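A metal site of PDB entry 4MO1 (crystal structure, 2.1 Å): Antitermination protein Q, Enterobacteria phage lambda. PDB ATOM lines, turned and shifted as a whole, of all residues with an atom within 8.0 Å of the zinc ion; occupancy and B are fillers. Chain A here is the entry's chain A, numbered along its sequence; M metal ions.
The backbone NH of Gly 114 sits close to the side-chain sulfur of Cys 110 (3.0 Å).
SG of Cys 110 sits close to N of Gly 112, 3.5 Å away.
The side-chain sulfur of Cys 110 lies close to the backbone NH of Val 113.
The side-chain sulfur of Cys 84 lies close to the backbone NH of Gly 88, at 3.0 Å.
N of Gly 86 lies close to SG of Cys 84 (3.6 Å).
N of Thr 87 lies close to SG of Cys 84, at 3.8 Å.
The backbone carbonyl oxygen of Gly 114 lies within hydrogen-bond range of the backbone NH of Cys 81 (3.2 Å).
N of Cys 107 is in hydrogen-bond range of O of Gly 88 (3.0 Å).
Of the 21 residues printed, 4 come within 4 Å of the zinc ion.
The nearest printed residue that does not touch the zinc ion is Gly 88 (4.3 Å).
The zinc ion is bound by SG of Cys 110 (2.4 Å), SG of Cys 84 (2.5 Å), SG of Cys 81 (2.5 Å) and SG of Cys 107 (2.6 Å).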
ATOM      1  N   ARG A  80     -21.629 -17.380 -25.129  1.00  0.00           N
ATOM      2  CA  ARG A  80     -22.771 -16.649 -24.578  1.00  0.00           C
ATOM      3  C   ARG A  80     -23.813 -16.502 -25.652  1.00  0.00           C
ATOM      4  O   ARG A  80     -23.481 -16.365 -26.831  1.00  0.00           O
ATOM      5  CB  ARG A  80     -22.399 -15.219 -24.150  1.00  0.00           C
ATOM      6  CG  ARG A  80     -21.466 -15.097 -22.984  1.00  0.00           C
ATOM      7  CD  ARG A  80     -21.715 -13.805 -22.215  1.00  0.00           C
ATOM      8  NE  ARG A  80     -21.370 -12.602 -22.960  1.00  0.00           N
ATOM      9  CZ  ARG A  80     -21.217 -11.414 -22.392  1.00  0.00           C
ATOM     10  NH1 ARG A  80     -21.379 -11.290 -21.074  1.00  0.00           N
ATOM     11  NH2 ARG A  80     -20.890 -10.356 -23.115  1.00  0.00           N
ATOM     12  N   CYS A  81     -25.075 -16.509 -25.258  1.00  0.00           N
ATOM     13  CA  CYS A  81     -26.135 -16.286 -26.219  1.00  0.00           C
ATOM     14  C   CYS A  81     -25.828 -14.900 -26.788  1.00  0.00           C
ATOM     15  O   CYS A  81     -25.368 -14.002 -26.074  1.00  0.00           O
ATOM     16  CB  CYS A  81     -27.509 -16.280 -25.537  1.00  0.00           C
ATOM     17  SG  CYS A  81     -28.790 -15.608 -26.569  1.00  0.00           S
ATOM     18  N   ARG A  82     -26.103 -14.719 -28.076  1.00  0.00           N
ATOM     19  CA  ARG A  82     -25.792 -13.456 -28.711  1.00  0.00           C
ATOM     20  C   ARG A  82     -26.932 -12.465 -28.625  1.00  0.00           C
ATOM     21  O   ARG A  82     -26.817 -11.355 -29.122  1.00  0.00           O
ATOM     22  CB  ARG A  82     -25.424 -13.702 -30.166  1.00  0.00           C
ATOM     23  CG  ARG A  82     -24.537 -14.933 -30.357  1.00  0.00           C
ATOM     24  CD  ARG A  82     -23.821 -14.897 -31.700  1.00  0.00           C
ATOM     25  NE  ARG A  82     -24.277 -15.922 -32.628  1.00  0.00           N
ATOM     26  CZ  ARG A  82     -23.953 -17.217 -32.542  1.00  0.00           C
ATOM     27  NH1 ARG A  82     -23.183 -17.650 -31.561  1.00  0.00           N
ATOM     28  NH2 ARG A  82     -24.405 -18.072 -33.458  1.00  0.00           N
ATOM     29  N   ASP A  83     -28.024 -12.866 -28.001  1.00  0.00           N
ATOM     30  CA  ASP A  83     -29.162 -11.965 -27.856  1.00  0.00           C
ATOM     31  C   ASP A  83     -29.163 -11.306 -26.485  1.00  0.00           C
ATOM     32  O   ASP A  83     -29.284 -10.087 -26.359  1.00  0.00           O
ATOM     33  CB  ASP A  83     -30.473 -12.729 -28.086  1.00  0.00           C
ATOM     34  CG  ASP A  83     -30.739 -13.012 -29.557  1.00  0.00           C
ATOM     35  OD1 ASP A  83     -31.110 -12.059 -30.288  1.00  0.00           O
ATOM     36  OD2 ASP A  83     -30.576 -14.170 -29.994  1.00  0.00           O
ATOM     37  N   CYS A  84     -29.023 -12.128 -25.441  1.00  0.00           N
ATOM     38  CA  CYS A  84     -29.057 -11.642 -24.073  1.00  0.00           C
ATOM     39  C   CYS A  84     -27.668 -11.423 -23.463  1.00  0.00           C
ATOM     40  O   CYS A  84     -27.538 -10.744 -22.443  1.00  0.00           O
ATOM     41  CB  CYS A  84     -29.859 -12.626 -23.208  1.00  0.00           C
ATOM     42  SG  CYS A  84     -29.078 -14.218 -22.937  1.00  0.00           S
ATOM     43  N   HIS A  85     -26.638 -11.987 -24.092  1.00  0.00           N
ATOM     44  CA  HIS A  85     -25.256 -11.880 -23.625  1.00  0.00           C
ATOM     45  C   HIS A  85     -25.079 -12.440 -22.211  1.00  0.00           C
ATOM     46  O   HIS A  85     -24.398 -11.845 -21.388  1.00  0.00           O
ATOM     47  CB  HIS A  85     -24.794 -10.418 -23.666  1.00  0.00           C
ATOM     48  CG  HIS A  85     -24.871  -9.811 -25.027  1.00  0.00           C
ATOM     49  ND1 HIS A  85     -24.116 -10.260 -26.085  1.00  0.00           N
ATOM     50  CD2 HIS A  85     -25.684  -8.840 -25.517  1.00  0.00           C
ATOM     51  CE1 HIS A  85     -24.464  -9.594 -27.179  1.00  0.00           C
ATOM     52  NE2 HIS A  85     -25.408  -8.731 -26.865  1.00  0.00           N
ATOM     53  N   GLY A  86     -25.706 -13.581 -21.964  1.00  0.00           N
ATOM     54  CA  GLY A  86     -25.568 -14.235 -20.671  1.00  0.00           C
ATOM     55  C   GLY A  86     -26.680 -14.104 -19.646  1.00  0.00           C
ATOM     56  O   GLY A  86     -26.814 -14.970 -18.788  1.00  0.00           O
ATOM     57  N   THR A  87     -27.478 -13.039 -19.716  1.00  0.00           N
ATOM     58  CA  THR A  87     -28.523 -12.873 -18.714  1.00  0.00           C
ATOM     59  C   THR A  87     -29.652 -13.879 -18.843  1.00  0.00           C
ATOM     60  O   THR A  87     -30.335 -14.193 -17.859  1.00  0.00           O
ATOM     61  CB  THR A  87     -29.145 -11.468 -18.770  1.00  0.00           C
ATOM     62  OG1 THR A  87     -29.986 -11.363 -19.925  1.00  0.00           O
ATOM     63  CG2 THR A  87     -28.049 -10.395 -18.824  1.00  0.00           C
ATOM     64  N   GLY A  88     -29.855 -14.380 -20.055  1.00  0.00           N
ATOM     65  CA  GLY A  88     -30.931 -15.325 -20.283  1.00  0.00           C
ATOM     66  C   GLY A  88     -32.284 -14.635 -20.209  1.00  0.00           C
ATOM     67  O   GLY A  88     -33.326 -15.298 -20.163  1.00  0.00           O
ATOM     68  N   ARG A  89     -32.269 -13.303 -20.227  1.00  0.00           N
ATOM     69  CA  ARG A  89     -33.485 -12.510 -20.151  1.00  0.00           C
ATOM     70  C   ARG A  89     -33.519 -11.428 -21.230  1.00  0.00           C
ATOM     71  O   ARG A  89     -32.494 -11.058 -21.795  1.00  0.00           O
ATOM     72  CB  ARG A  89     -33.598 -11.839 -18.774  1.00  0.00           C
ATOM     73  CG  ARG A  89     -33.458 -12.805 -17.597  1.00  0.00           C
ATOM     74  CD  ARG A  89     -34.686 -13.676 -17.434  1.00  0.00           C
ATOM     75  NE  ARG A  89     -35.788 -12.940 -16.814  1.00  0.00           N
ATOM     76  CZ  ARG A  89     -37.038 -13.380 -16.728  1.00  0.00           C
ATOM     77  NH1 ARG A  89     -37.367 -14.552 -17.232  1.00  0.00           N
ATOM     78  NH2 ARG A  89     -37.962 -12.635 -16.136  1.00  0.00           N
ATOM     79  N   ALA A  90     -34.724 -10.918 -21.472  1.00  0.00           N
ATOM     80  CA  ALA A  90     -34.930  -9.851 -22.441  1.00  0.00           C
ATOM     81  C   ALA A  90     -36.022  -8.962 -21.863  1.00  0.00           C
ATOM     82  O   ALA A  90     -36.731  -9.366 -20.946  1.00  0.00           O
ATOM     83  CB  ALA A  90     -35.380 -10.449 -23.773  1.00  0.00           C
ATOM     84  N   GLU A 106     -38.174 -14.280 -20.459  1.00  0.00           N
ATOM     85  CA  GLU A 106     -37.120 -15.207 -20.839  1.00  0.00           C
ATOM     86  C   GLU A 106     -36.575 -14.841 -22.216  1.00  0.00           C
ATOM     87  O   GLU A 106     -37.292 -14.272 -23.049  1.00  0.00           O
ATOM     88  CB  GLU A 106     -37.660 -16.635 -20.865  1.00  0.00           C
ATOM     89  CG  GLU A 106     -36.655 -17.684 -21.298  1.00  0.00           C
ATOM     90  CD  GLU A 106     -37.250 -19.070 -21.370  1.00  0.00           C
ATOM     91  OE1 GLU A 106     -37.788 -19.438 -22.440  1.00  0.00           O
ATOM     92  OE2 GLU A 106     -37.211 -19.785 -20.351  1.00  0.00           O
ATOM     93  N   CYS A 107     -35.306 -15.142 -22.459  1.00  0.00           N
ATOM     94  CA  CYS A 107     -34.727 -14.905 -23.763  1.00  0.00           C
ATOM     95  C   CYS A 107     -35.077 -16.168 -24.524  1.00  0.00           C
ATOM     96  O   CYS A 107     -34.745 -17.273 -24.098  1.00  0.00           O
ATOM     97  CB  CYS A 107     -33.210 -14.754 -23.674  1.00  0.00           C
ATOM     98  SG  CYS A 107     -32.404 -14.388 -25.261  1.00  0.00           S
ATOM     99  N   GLY A 108     -35.783 -16.019 -25.640  1.00  0.00           N
ATOM    100  CA  GLY A 108     -36.176 -17.178 -26.405  1.00  0.00           C
ATOM    101  C   GLY A 108     -35.010 -17.915 -27.046  1.00  0.00           C
ATOM    102  O   GLY A 108     -34.975 -19.149 -27.050  1.00  0.00           O
ATOM    103  N   ARG A 109     -34.045 -17.162 -27.564  1.00  0.00           N
ATOM    104  CA  ARG A 109     -32.892 -17.741 -28.243  1.00  0.00           C
ATOM    105  C   ARG A 109     -32.180 -18.820 -27.437  1.00  0.00           C
ATOM    106  O   ARG A 109     -31.885 -19.898 -27.955  1.00  0.00           O
ATOM    107  CB  ARG A 109     -31.925 -16.648 -28.635  1.00  0.00           C
ATOM    108  N   CYS A 110     -31.886 -18.536 -26.171  1.00  0.00           N
ATOM    109  CA  CYS A 110     -31.193 -19.518 -25.350  1.00  0.00           C
ATOM    110  C   CYS A 110     -32.134 -20.148 -24.333  1.00  0.00           C
ATOM    111  O   CYS A 110     -31.714 -20.914 -23.462  1.00  0.00           O
ATOM    112  CB  CYS A 110     -30.018 -18.870 -24.619  1.00  0.00           C
ATOM    113  SG  CYS A 110     -30.465 -17.710 -23.305  1.00  0.00           S
ATOM    114  N   LYS A 111     -33.418 -19.815 -24.459  1.00  0.00           N
ATOM    115  CA  LYS A 111     -34.443 -20.329 -23.565  1.00  0.00           C
ATOM    116  C   LYS A 111     -34.054 -20.063 -22.120  1.00  0.00           C
ATOM    117  O   LYS A 111     -34.277 -20.902 -21.248  1.00  0.00           O
ATOM    118  CB  LYS A 111     -34.654 -21.816 -23.801  1.00  0.00           C
ATOM    119  N   GLY A 112     -33.464 -18.902 -21.875  1.00  0.00           N
ATOM    120  CA  GLY A 112     -33.067 -18.522 -20.533  1.00  0.00           C
ATOM    121  C   GLY A 112     -31.827 -19.180 -19.975  1.00  0.00           C
ATOM    122  O   GLY A 112     -31.559 -19.063 -18.777  1.00  0.00           O
ATOM    123  N   VAL A 113     -31.053 -19.871 -20.804  1.00  0.00           N
ATOM    124  CA  VAL A 113     -29.838 -20.504 -20.313  1.00  0.00           C
ATOM    125  C   VAL A 113     -28.636 -19.538 -20.248  1.00  0.00           C
ATOM    126  O   VAL A 113     -27.832 -19.608 -19.323  1.00  0.00           O
ATOM    127  CB  VAL A 113     -29.477 -21.747 -21.149  1.00  0.00           C
ATOM    128  CG1 VAL A 113     -28.120 -22.287 -20.722  1.00  0.00           C
ATOM    129  CG2 VAL A 113     -30.539 -22.813 -20.947  1.00  0.00           C
ATOM    130  N   GLY A 114     -28.515 -18.657 -21.231  1.00  0.00           N
ATOM    131  CA  GLY A 114     -27.447 -17.668 -21.230  1.00  0.00           C
ATOM    132  C   GLY A 114     -26.010 -18.110 -21.398  1.00  0.00           C
ATOM    133  O   GLY A 114     -25.351 -17.714 -22.352  1.00  0.00           O
ATOM    134  N   TYR A 115     -25.495 -18.908 -20.461  1.00  0.00           N
ATOM    135  CA  TYR A 115     -24.097 -19.360 -20.539  1.00  0.00           C
ATOM    136  C   TYR A 115     -23.959 -20.866 -20.288  1.00  0.00           C
ATOM    137  O   TYR A 115     -24.827 -21.471 -19.642  1.00  0.00           O
ATOM    138  CB  TYR A 115     -23.244 -18.600 -19.529  1.00  0.00           C
ATOM    139  CG  TYR A 115     -23.743 -18.746 -18.109  1.00  0.00           C
ATOM    140  CD1 TYR A 115     -24.803 -17.953 -17.640  1.00  0.00           C
ATOM    141  CD2 TYR A 115     -23.215 -19.708 -17.257  1.00  0.00           C
ATOM    142  CE1 TYR A 115     -25.317 -18.132 -16.369  1.00  0.00           C
ATOM    143  CE2 TYR A 115     -23.717 -19.887 -15.970  1.00  0.00           C
ATOM    144  CZ  TYR A 115     -24.771 -19.099 -15.530  1.00  0.00           C
ATOM    145  OH  TYR A 115     -25.279 -19.276 -14.275  1.00  0.00           O
HETATM  146 ZN    ZN M   1     -30.286 -15.675 -24.549  1.00  0.00          ZN
